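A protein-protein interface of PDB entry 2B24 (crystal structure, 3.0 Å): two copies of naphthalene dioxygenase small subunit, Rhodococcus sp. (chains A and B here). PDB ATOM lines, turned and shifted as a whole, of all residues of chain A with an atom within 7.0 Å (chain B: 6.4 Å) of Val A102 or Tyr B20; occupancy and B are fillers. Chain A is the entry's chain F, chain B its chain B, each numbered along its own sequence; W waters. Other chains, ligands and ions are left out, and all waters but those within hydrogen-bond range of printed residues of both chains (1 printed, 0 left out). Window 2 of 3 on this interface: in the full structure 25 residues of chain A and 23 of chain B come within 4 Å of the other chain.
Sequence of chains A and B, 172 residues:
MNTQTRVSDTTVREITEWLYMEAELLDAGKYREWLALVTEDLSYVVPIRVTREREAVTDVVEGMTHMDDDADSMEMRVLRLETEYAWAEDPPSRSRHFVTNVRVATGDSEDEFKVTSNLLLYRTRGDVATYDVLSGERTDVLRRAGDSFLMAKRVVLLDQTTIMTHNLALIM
OE1 of Glu B24 is in salt-bridge range of NH1 of Arg A103.
The backbone NH (N) of Val B99 lies close to the side-chain amide nitrogen (ND2) of Asn A101, at 3.1 Å.
Water W1 lies within hydrogen-bond range of O of Val B99, OH of Tyr B20 and N of Asn A101.
Among the printed residues, pairs that only touch across the chains: Val A102 with Tyr B20, Asn A101 with Ala B23, Arg A103 with Tyr B20, Asn A101 with Tyr B20 and Thr A100 with Thr B100.
Thr B100 touches its own counterpart, Thr A100.
Val A102 touches Tyr B20, but with the chains exchanged Tyr A20 does not touch Val B102 (10.0 Å).
Of the 7 pairs that touch across the chains among the printed residues, 1 has its exchanged pair printed and touching as well.
OD1 of Asn A118 sits at hydrogen-bond distance from NH2 of Arg A103 (2.9 Å).
The guanidinium group (NE) of Arg A103 sits at hydrogen-bond distance from the backbone carbonyl oxygen (O) of Asn A101.
The side-chain amide nitrogen (ND2) of Asn A101 sits at hydrogen-bond distance from the side-chain hydroxyl (OG1) of Thr A100, at 2.8 Å.
N of Arg A103 lies within hydrogen-bond range of O of Thr A116 (2.9 Å).
The backbone NH (N) of Asn A118 is in hydrogen-bond range of the backbone carbonyl oxygen (O) of Thr A100 (2.9 Å).
Printed residues of chain A within 4 Å of Tyr B20: Asn A101 (3.9 Å), Val A102 (3.5 Å) and Arg A103 (3.9 Å).
Of the printed residues of chain A, Glu B24 touches Arg A103.
Printed residues of chain A within 4 Å of Val B99: Asn A101 (3.1 Å).
Printed residues of chain A within 4 Å of Thr B100: Thr A100 (3.98 Å).
Asp B27 touches none of the printed residues of chain A.
The nearest residue of chain B that does not touch Val A102 is Glu B17 (5.2 Å).
Of the 16 printed residues of chain A, 4 touch a printed residue of chain B.
Hydrophobic or aromatic side chains of chain B that line the printed part of chain A: Tyr B20, Ala B23 and Val B99.
Along chain B the printed residues that touch a printed residue of chain A span positions 20 to 100.
Among the printed residues, Asp or Glu carboxylates within 4 Å of a Lys or Arg side-chain nitrogen of the other chain: Arg A103 with Glu B24 (2.9 Å).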
ATOM      1  N   VAL A  12      12.347  20.817  18.258  1.00  0.00           N
ATOM      2  CA  VAL A  12      10.982  20.804  18.764  1.00  0.00           C
ATOM      3  C   VAL A  12      11.017  20.747  20.299  1.00  0.00           C
ATOM      4  O   VAL A  12      10.473  21.622  20.960  1.00  0.00           O
ATOM      5  CB  VAL A  12      10.170  19.645  18.162  1.00  0.00           C
ATOM      6  CG1 VAL A  12       8.832  19.518  18.842  1.00  0.00           C
ATOM      7  CG2 VAL A  12       9.974  19.855  16.685  1.00  0.00           C
ATOM      8  N   ILE A  15      12.271  24.266  21.533  1.00  0.00           N
ATOM      9  CA  ILE A  15      11.358  25.388  21.304  1.00  0.00           C
ATOM     10  C   ILE A  15      10.079  25.226  22.138  1.00  0.00           C
ATOM     11  O   ILE A  15       9.559  26.199  22.668  1.00  0.00           O
ATOM     12  CB  ILE A  15      11.028  25.521  19.802  1.00  0.00           C
ATOM     13  CG1 ILE A  15      12.195  26.158  19.058  1.00  0.00           C
ATOM     14  CG2 ILE A  15       9.784  26.340  19.598  1.00  0.00           C
ATOM     15  CD1 ILE A  15      12.218  25.894  17.593  1.00  0.00           C
ATOM     16  N   THR A  16       9.588  23.995  22.246  1.00  0.00           N
ATOM     17  CA  THR A  16       8.425  23.687  23.070  1.00  0.00           C
ATOM     18  C   THR A  16       8.669  24.017  24.540  1.00  0.00           C
ATOM     19  O   THR A  16       7.813  24.584  25.182  1.00  0.00           O
ATOM     20  CB  THR A  16       8.024  22.207  22.905  1.00  0.00           C
ATOM     21  OG1 THR A  16       7.510  21.994  21.585  1.00  0.00           O
ATOM     22  CG2 THR A  16       6.856  21.864  23.781  1.00  0.00           C
ATOM     23  N   LEU A  19       8.791  27.770  25.101  1.00  0.00           N
ATOM     24  CA  LEU A  19       7.457  28.343  25.162  1.00  0.00           C
ATOM     25  C   LEU A  19       6.760  28.086  26.479  1.00  0.00           C
ATOM     26  O   LEU A  19       5.876  28.856  26.851  1.00  0.00           O
ATOM     27  CB  LEU A  19       6.575  27.834  24.022  1.00  0.00           C
ATOM     28  CG  LEU A  19       6.857  28.220  22.564  1.00  0.00           C
ATOM     29  CD1 LEU A  19       5.780  27.627  21.685  1.00  0.00           C
ATOM     30  CD2 LEU A  19       6.986  29.725  22.344  1.00  0.00           C
ATOM     31  N   TYR A  20       7.144  27.015  27.173  1.00  0.00           N
ATOM     32  CA  TYR A  20       6.619  26.715  28.510  1.00  0.00           C
ATOM     33  C   TYR A  20       7.324  27.531  29.586  1.00  0.00           C
ATOM     34  O   TYR A  20       6.727  27.880  30.591  1.00  0.00           O
ATOM     35  CB  TYR A  20       6.759  25.234  28.838  1.00  0.00           C
ATOM     36  CG  TYR A  20       5.974  24.296  27.955  1.00  0.00           C
ATOM     37  CD1 TYR A  20       6.178  22.926  28.015  1.00  0.00           C
ATOM     38  CD2 TYR A  20       5.037  24.771  27.057  1.00  0.00           C
ATOM     39  CE1 TYR A  20       5.471  22.053  27.191  1.00  0.00           C
ATOM     40  CE2 TYR A  20       4.322  23.906  26.231  1.00  0.00           C
ATOM     41  CZ  TYR A  20       4.545  22.556  26.308  1.00  0.00           C
ATOM     42  OH  TYR A  20       3.822  21.727  25.508  1.00  0.00           O
ATOM     43  N   VAL A  99      -0.400  27.075  26.853  1.00  0.00           N
ATOM     44  CA  VAL A  99       0.237  26.913  25.541  1.00  0.00           C
ATOM     45  C   VAL A  99       0.064  25.499  25.022  1.00  0.00           C
ATOM     46  O   VAL A  99       0.669  24.570  25.532  1.00  0.00           O
ATOM     47  CB  VAL A  99       1.749  27.187  25.612  1.00  0.00           C
ATOM     48  CG1 VAL A  99       2.334  27.244  24.232  1.00  0.00           C
ATOM     49  CG2 VAL A  99       2.043  28.471  26.372  1.00  0.00           C
ATOM     50  N   THR A 100      -0.757  25.333  24.007  1.00  0.00           N
ATOM     51  CA  THR A 100      -1.051  24.021  23.475  1.00  0.00           C
ATOM     52  C   THR A 100      -0.811  24.019  21.977  1.00  0.00           C
ATOM     53  O   THR A 100      -0.365  25.004  21.436  1.00  0.00           O
ATOM     54  CB  THR A 100      -2.492  23.614  23.818  1.00  0.00           C
ATOM     55  OG1 THR A 100      -3.408  24.350  23.010  1.00  0.00           O
ATOM     56  CG2 THR A 100      -2.870  24.046  25.222  1.00  0.00           C
ATOM     57  N   ASN A 101      -1.090  22.909  21.308  1.00  0.00           N
ATOM     58  CA  ASN A 101      -0.907  22.780  19.855  1.00  0.00           C
ATOM     59  C   ASN A 101       0.361  23.440  19.272  1.00  0.00           C
ATOM     60  O   ASN A 101       0.278  24.192  18.310  1.00  0.00           O
ATOM     61  CB  ASN A 101      -2.122  23.325  19.109  1.00  0.00           C
ATOM     62  CG  ASN A 101      -3.421  22.666  19.501  1.00  0.00           C
ATOM     63  OD1 ASN A 101      -4.179  22.258  18.633  1.00  0.00           O
ATOM     64  ND2 ASN A 101      -3.712  22.605  20.796  1.00  0.00           N
ATOM     65  N   VAL A 102       1.531  23.159  19.840  1.00  0.00           N
ATOM     66  CA  VAL A 102       2.772  23.756  19.338  1.00  0.00           C
ATOM     67  C   VAL A 102       3.229  23.096  18.041  1.00  0.00           C
ATOM     68  O   VAL A 102       3.420  21.886  17.978  1.00  0.00           O
ATOM     69  CB  VAL A 102       3.917  23.733  20.373  1.00  0.00           C
ATOM     70  CG1 VAL A 102       5.097  24.553  19.869  1.00  0.00           C
ATOM     71  CG2 VAL A 102       3.458  24.265  21.730  1.00  0.00           C
ATOM     72  N   ARG A 103       3.392  23.917  17.009  1.00  0.00           N
ATOM     73  CA  ARG A 103       3.767  23.471  15.675  1.00  0.00           C
ATOM     74  C   ARG A 103       5.016  24.207  15.249  1.00  0.00           C
ATOM     75  O   ARG A 103       4.951  25.391  14.948  1.00  0.00           O
ATOM     76  CB  ARG A 103       2.644  23.766  14.689  1.00  0.00           C
ATOM     77  CG  ARG A 103       1.370  22.997  14.965  1.00  0.00           C
ATOM     78  CD  ARG A 103       0.101  23.713  14.581  1.00  0.00           C
ATOM     79  NE  ARG A 103      -0.380  24.592  15.640  1.00  0.00           N
ATOM     80  CZ  ARG A 103      -1.090  25.684  15.429  1.00  0.00           C
ATOM     81  NH1 ARG A 103      -1.406  26.041  14.207  1.00  0.00           N
ATOM     82  NH2 ARG A 103      -1.480  26.433  16.435  1.00  0.00           N
ATOM     83  N   VAL A 104       6.152  23.509  15.238  1.00  0.00           N
ATOM     84  CA  VAL A 104       7.435  24.106  14.855  1.00  0.00           C
ATOM     85  C   VAL A 104       7.767  23.796  13.396  1.00  0.00           C
ATOM     86  O   VAL A 104       7.654  22.660  12.950  1.00  0.00           O
ATOM     87  CB  VAL A 104       8.594  23.642  15.763  1.00  0.00           C
ATOM     88  CG1 VAL A 104       9.779  24.548  15.593  1.00  0.00           C
ATOM     89  CG2 VAL A 104       8.181  23.607  17.219  1.00  0.00           C
ATOM     90  N   VAL A 115       7.077  29.498  14.891  1.00  0.00           N
ATOM     91  CA  VAL A 115       6.549  28.737  16.012  1.00  0.00           C
ATOM     92  C   VAL A 115       5.099  29.116  16.333  1.00  0.00           C
ATOM     93  O   VAL A 115       4.839  30.169  16.917  1.00  0.00           O
ATOM     94  CB  VAL A 115       7.417  28.926  17.266  1.00  0.00           C
ATOM     95  CG1 VAL A 115       7.055  27.907  18.308  1.00  0.00           C
ATOM     96  CG2 VAL A 115       8.867  28.831  16.921  1.00  0.00           C
ATOM     97  N   THR A 116       4.162  28.238  15.979  1.00  0.00           N
ATOM     98  CA  THR A 116       2.742  28.496  16.170  1.00  0.00           C
ATOM     99  C   THR A 116       2.175  27.735  17.368  1.00  0.00           C
ATOM    100  O   THR A 116       2.314  26.529  17.453  1.00  0.00           O
ATOM    101  CB  THR A 116       1.975  28.131  14.896  1.00  0.00           C
ATOM    102  OG1 THR A 116       2.833  28.265  13.759  1.00  0.00           O
ATOM    103  CG2 THR A 116       0.918  29.141  14.628  1.00  0.00           C
ATOM    104  N   SER A 117       1.543  28.444  18.297  1.00  0.00           N
ATOM    105  CA  SER A 117       0.910  27.835  19.465  1.00  0.00           C
ATOM    106  C   SER A 117      -0.524  28.311  19.617  1.00  0.00           C
ATOM    107  O   SER A 117      -0.899  29.339  19.080  1.00  0.00           O
ATOM    108  CB  SER A 117       1.678  28.192  20.728  1.00  0.00           C
ATOM    109  OG  SER A 117       2.561  29.281  20.528  1.00  0.00           O
ATOM    110  N   ASN A 118      -1.330  27.555  20.345  1.00  0.00           N
ATOM    111  CA  ASN A 118      -2.664  27.991  20.731  1.00  0.00           C
ATOM    112  C   ASN A 118      -2.616  28.482  22.141  1.00  0.00           C
ATOM    113  O   ASN A 118      -2.132  27.798  23.000  1.00  0.00           O
ATOM    114  CB  ASN A 118      -3.643  26.832  20.669  1.00  0.00           C
ATOM    115  CG  ASN A 118      -4.072  26.521  19.290  1.00  0.00           C
ATOM    116  OD1 ASN A 118      -3.551  27.066  18.349  1.00  0.00           O
ATOM    117  ND2 ASN A 118      -5.028  25.628  19.159  1.00  0.00           N
ATOM    118  N   ARG A 138      -0.880  32.234  18.637  1.00  0.00           N
ATOM    119  CA  ARG A 138       0.336  33.010  18.441  1.00  0.00           C
ATOM    120  C   ARG A 138       1.152  32.436  17.310  1.00  0.00           C
ATOM    121  O   ARG A 138       1.335  31.241  17.244  1.00  0.00           O
ATOM    122  CB  ARG A 138       1.166  33.063  19.708  1.00  0.00           C
ATOM    123  CG  ARG A 138       0.391  33.355  20.974  1.00  0.00           C
ATOM    124  CD  ARG A 138       0.534  32.267  22.005  1.00  0.00           C
ATOM    125  NE  ARG A 138       1.484  32.589  23.063  1.00  0.00           N
ATOM    126  CZ  ARG A 138       2.292  31.718  23.631  1.00  0.00           C
ATOM    127  NH1 ARG A 138       2.301  30.452  23.243  1.00  0.00           N
ATOM    128  NH2 ARG A 138       3.096  32.121  24.592  1.00  0.00           N
ATOM    129  N   ILE B  15       1.805  11.357  14.957  1.00  0.00           N
ATOM    130  CA  ILE B  15       0.374  11.369  15.202  1.00  0.00           C
ATOM    131  C   ILE B  15      -0.011  12.653  15.918  1.00  0.00           C
ATOM    132  O   ILE B  15      -1.025  13.256  15.611  1.00  0.00           O
ATOM    133  CB  ILE B  15      -0.038  10.125  15.997  1.00  0.00           C
ATOM    134  CG1 ILE B  15      -0.151   8.933  15.044  1.00  0.00           C
ATOM    135  CG2 ILE B  15      -1.357  10.353  16.678  1.00  0.00           C
ATOM    136  CD1 ILE B  15      -0.081   7.581  15.692  1.00  0.00           C
ATOM    137  N   THR B  16       0.824  13.077  16.859  1.00  0.00           N
ATOM    138  CA  THR B  16       0.608  14.313  17.607  1.00  0.00           C
ATOM    139  C   THR B  16       0.603  15.528  16.690  1.00  0.00           C
ATOM    140  O   THR B  16      -0.255  16.387  16.813  1.00  0.00           O
ATOM    141  CB  THR B  16       1.649  14.459  18.712  1.00  0.00           C
ATOM    142  OG1 THR B  16       1.408  13.473  19.722  1.00  0.00           O
ATOM    143  CG2 THR B  16       1.439  15.724  19.455  1.00  0.00           C
ATOM    144  N   GLU B  17       1.544  15.581  15.758  1.00  0.00           N
ATOM    145  CA  GLU B  17       1.616  16.676  14.791  1.00  0.00           C
ATOM    146  C   GLU B  17       0.536  16.589  13.707  1.00  0.00           C
ATOM    147  O   GLU B  17       0.229  17.575  13.042  1.00  0.00           O
ATOM    148  CB  GLU B  17       3.010  16.759  14.172  1.00  0.00           C
ATOM    149  CG  GLU B  17       4.084  17.121  15.182  1.00  0.00           C
ATOM    150  CD  GLU B  17       5.406  17.516  14.548  1.00  0.00           C
ATOM    151  OE1 GLU B  17       6.079  18.428  15.091  1.00  0.00           O
ATOM    152  OE2 GLU B  17       5.780  16.913  13.518  1.00  0.00           O
ATOM    153  N   TRP B  18      -0.039  15.408  13.530  1.00  0.00           N
ATOM    154  CA  TRP B  18      -1.177  15.228  12.639  1.00  0.00           C
ATOM    155  C   TRP B  18      -2.396  15.894  13.282  1.00  0.00           C
ATOM    156  O   TRP B  18      -3.076  16.696  12.648  1.00  0.00           O
ATOM    157  CB  TRP B  18      -1.422  13.735  12.410  1.00  0.00           C
ATOM    158  CG  TRP B  18      -2.396  13.404  11.334  1.00  0.00           C
ATOM    159  CD1 TRP B  18      -2.115  13.180  10.026  1.00  0.00           C
ATOM    160  CD2 TRP B  18      -3.813  13.231  11.471  1.00  0.00           C
ATOM    161  NE1 TRP B  18      -3.266  12.889   9.332  1.00  0.00           N
ATOM    162  CE2 TRP B  18      -4.321  12.913  10.199  1.00  0.00           C
ATOM    163  CE3 TRP B  18      -4.711  13.311  12.547  1.00  0.00           C
ATOM    164  CZ2 TRP B  18      -5.669  12.675   9.974  1.00  0.00           C
ATOM    165  CZ3 TRP B  18      -6.052  13.079  12.312  1.00  0.00           C
ATOM    166  CH2 TRP B  18      -6.516  12.765  11.043  1.00  0.00           C
ATOM    167  N   LEU B  19      -2.632  15.575  14.556  1.00  0.00           N
ATOM    168  CA  LEU B  19      -3.737  16.119  15.340  1.00  0.00           C
ATOM    169  C   LEU B  19      -3.694  17.639  15.482  1.00  0.00           C
ATOM    170  O   LEU B  19      -4.739  18.270  15.649  1.00  0.00           O
ATOM    171  CB  LEU B  19      -3.784  15.489  16.728  1.00  0.00           C
ATOM    172  CG  LEU B  19      -4.090  14.000  16.870  1.00  0.00           C
ATOM    173  CD1 LEU B  19      -4.221  13.697  18.335  1.00  0.00           C
ATOM    174  CD2 LEU B  19      -5.355  13.572  16.110  1.00  0.00           C
ATOM    175  N   TYR B  20      -2.496  18.221  15.423  1.00  0.00           N
ATOM    176  CA  TYR B  20      -2.328  19.666  15.463  1.00  0.00           C
ATOM    177  C   TYR B  20      -2.567  20.287  14.093  1.00  0.00           C
ATOM    178  O   TYR B  20      -3.053  21.412  13.988  1.00  0.00           O
ATOM    179  CB  TYR B  20      -0.927  20.032  15.942  1.00  0.00           C
ATOM    180  CG  TYR B  20      -0.601  19.639  17.367  1.00  0.00           C
ATOM    181  CD1 TYR B  20       0.695  19.759  17.854  1.00  0.00           C
ATOM    182  CD2 TYR B  20      -1.580  19.158  18.231  1.00  0.00           C
ATOM    183  CE1 TYR B  20       1.001  19.401  19.154  1.00  0.00           C
ATOM    184  CE2 TYR B  20      -1.275  18.797  19.535  1.00  0.00           C
ATOM    185  CZ  TYR B  20       0.007  18.923  19.983  1.00  0.00           C
ATOM    186  OH  TYR B  20       0.306  18.562  21.260  1.00  0.00           O
ATOM    187  N   MET B  21      -2.211  19.555  13.042  1.00  0.00           N
ATOM    188  CA  MET B  21      -2.416  20.014  11.676  1.00  0.00           C
ATOM    189  C   MET B  21      -3.873  19.905  11.312  1.00  0.00           C
ATOM    190  O   MET B  21      -4.388  20.763  10.612  1.00  0.00           O
ATOM    191  CB  MET B  21      -1.576  19.203  10.688  1.00  0.00           C
ATOM    192  CG  MET B  21      -2.054  19.276   9.240  1.00  0.00           C
ATOM    193  SD  MET B  21      -2.699  17.707   8.648  1.00  0.00           S
ATOM    194  CE  MET B  21      -1.213  17.126   7.728  1.00  0.00           C
ATOM    195  N   GLU B  22      -4.522  18.840  11.775  1.00  0.00           N
ATOM    196  CA  GLU B  22      -5.965  18.660  11.628  1.00  0.00           C
ATOM    197  C   GLU B  22      -6.732  19.797  12.302  1.00  0.00           C
ATOM    198  O   GLU B  22      -7.643  20.347  11.711  1.00  0.00           O
ATOM    199  CB  GLU B  22      -6.375  17.321  12.226  1.00  0.00           C
ATOM    200  CG  GLU B  22      -7.809  16.920  11.986  1.00  0.00           C
ATOM    201  CD  GLU B  22      -8.463  16.335  13.213  1.00  0.00           C
ATOM    202  OE1 GLU B  22      -7.835  16.313  14.294  1.00  0.00           O
ATOM    203  OE2 GLU B  22      -9.619  15.897  13.088  1.00  0.00           O
ATOM    204  N   ALA B  23      -6.346  20.142  13.532  1.00  0.00           N
ATOM    205  CA  ALA B  23      -6.906  21.281  14.256  1.00  0.00           C
ATOM    206  C   ALA B  23      -6.638  22.604  13.554  1.00  0.00           C
ATOM    207  O   ALA B  23      -7.500  23.467  13.541  1.00  0.00           O
ATOM    208  CB  ALA B  23      -6.376  21.328  15.686  1.00  0.00           C
ATOM    209  N   GLU B  24      -5.450  22.750  12.974  1.00  0.00           N
ATOM    210  CA  GLU B  24      -5.044  23.972  12.275  1.00  0.00           C
ATOM    211  C   GLU B  24      -5.862  24.215  11.017  1.00  0.00           C
ATOM    212  O   GLU B  24      -6.053  25.354  10.612  1.00  0.00           O
ATOM    213  CB  GLU B  24      -3.556  23.906  11.922  1.00  0.00           C
ATOM    214  CG  GLU B  24      -2.953  25.203  11.399  1.00  0.00           C
ATOM    215  CD  GLU B  24      -1.526  25.039  10.906  1.00  0.00           C
ATOM    216  OE1 GLU B  24      -0.646  24.736  11.713  1.00  0.00           O
ATOM    217  OE2 GLU B  24      -1.271  25.218   9.712  1.00  0.00           O
ATOM    218  N   LEU B  25      -6.330  23.128  10.411  1.00  0.00           N
ATOM    219  CA  LEU B  25      -7.167  23.161   9.229  1.00  0.00           C
ATOM    220  C   LEU B  25      -8.589  23.508   9.591  1.00  0.00           C
ATOM    221  O   LEU B  25      -9.235  24.242   8.872  1.00  0.00           O
ATOM    222  CB  LEU B  25      -7.147  21.805   8.541  1.00  0.00           C
ATOM    223  CG  LEU B  25      -6.540  21.669   7.146  1.00  0.00           C
ATOM    224  CD1 LEU B  25      -5.155  22.277   7.081  1.00  0.00           C
ATOM    225  CD2 LEU B  25      -6.485  20.211   6.763  1.00  0.00           C
ATOM    226  N   ASP B  27      -9.759  25.120  12.495  1.00  0.00           N
ATOM    227  CA  ASP B  27      -9.826  26.508  12.971  1.00  0.00           C
ATOM    228  C   ASP B  27      -9.591  27.550  11.890  1.00  0.00           C
ATOM    229  O   ASP B  27      -9.766  28.730  12.140  1.00  0.00           O
ATOM    230  CB  ASP B  27      -8.782  26.770  14.039  1.00  0.00           C
ATOM    231  CG  ASP B  27      -8.807  25.779  15.129  1.00  0.00           C
ATOM    232  OD1 ASP B  27      -9.902  25.378  15.530  1.00  0.00           O
ATOM    233  OD2 ASP B  27      -7.758  25.370  15.660  1.00  0.00           O
ATOM    234  N   VAL B  99      -6.190  20.860  21.422  1.00  0.00           N
ATOM    235  CA  VAL B  99      -5.874  19.437  21.512  1.00  0.00           C
ATOM    236  C   VAL B  99      -4.799  19.188  22.555  1.00  0.00           C
ATOM    237  O   VAL B  99      -3.630  19.518  22.341  1.00  0.00           O
ATOM    238  CB  VAL B  99      -5.395  18.856  20.194  1.00  0.00           C
ATOM    239  CG1 VAL B  99      -5.363  17.371  20.310  1.00  0.00           C
ATOM    240  CG2 VAL B  99      -6.290  19.250  19.074  1.00  0.00           C
ATOM    241  N   THR B 100      -5.193  18.611  23.687  1.00  0.00           N
ATOM    242  CA  THR B 100      -4.247  18.324  24.758  1.00  0.00           C
ATOM    243  C   THR B 100      -4.312  16.842  25.147  1.00  0.00           C
ATOM    244  O   THR B 100      -5.076  16.092  24.561  1.00  0.00           O
ATOM    245  CB  THR B 100      -4.511  19.232  25.956  1.00  0.00           C
ATOM    246  OG1 THR B 100      -5.697  18.797  26.622  1.00  0.00           O
ATOM    247  CG2 THR B 100      -4.864  20.614  25.516  1.00  0.00           C
ATOM    248  N   VAL B 102      -2.663  14.094  24.528  1.00  0.00           N
ATOM    249  CA  VAL B 102      -2.623  13.075  23.482  1.00  0.00           C
ATOM    250  C   VAL B 102      -1.988  11.758  23.965  1.00  0.00           C
ATOM    251  O   VAL B 102      -0.857  11.730  24.445  1.00  0.00           O
ATOM    252  CB  VAL B 102      -1.912  13.575  22.199  1.00  0.00           C
ATOM    253  CG1 VAL B 102      -2.079  12.566  21.061  1.00  0.00           C
ATOM    254  CG2 VAL B 102      -2.440  14.928  21.773  1.00  0.00           C
HETATM  255  O   HOH W   1      -1.267  19.956  22.995  1.00  0.00           O
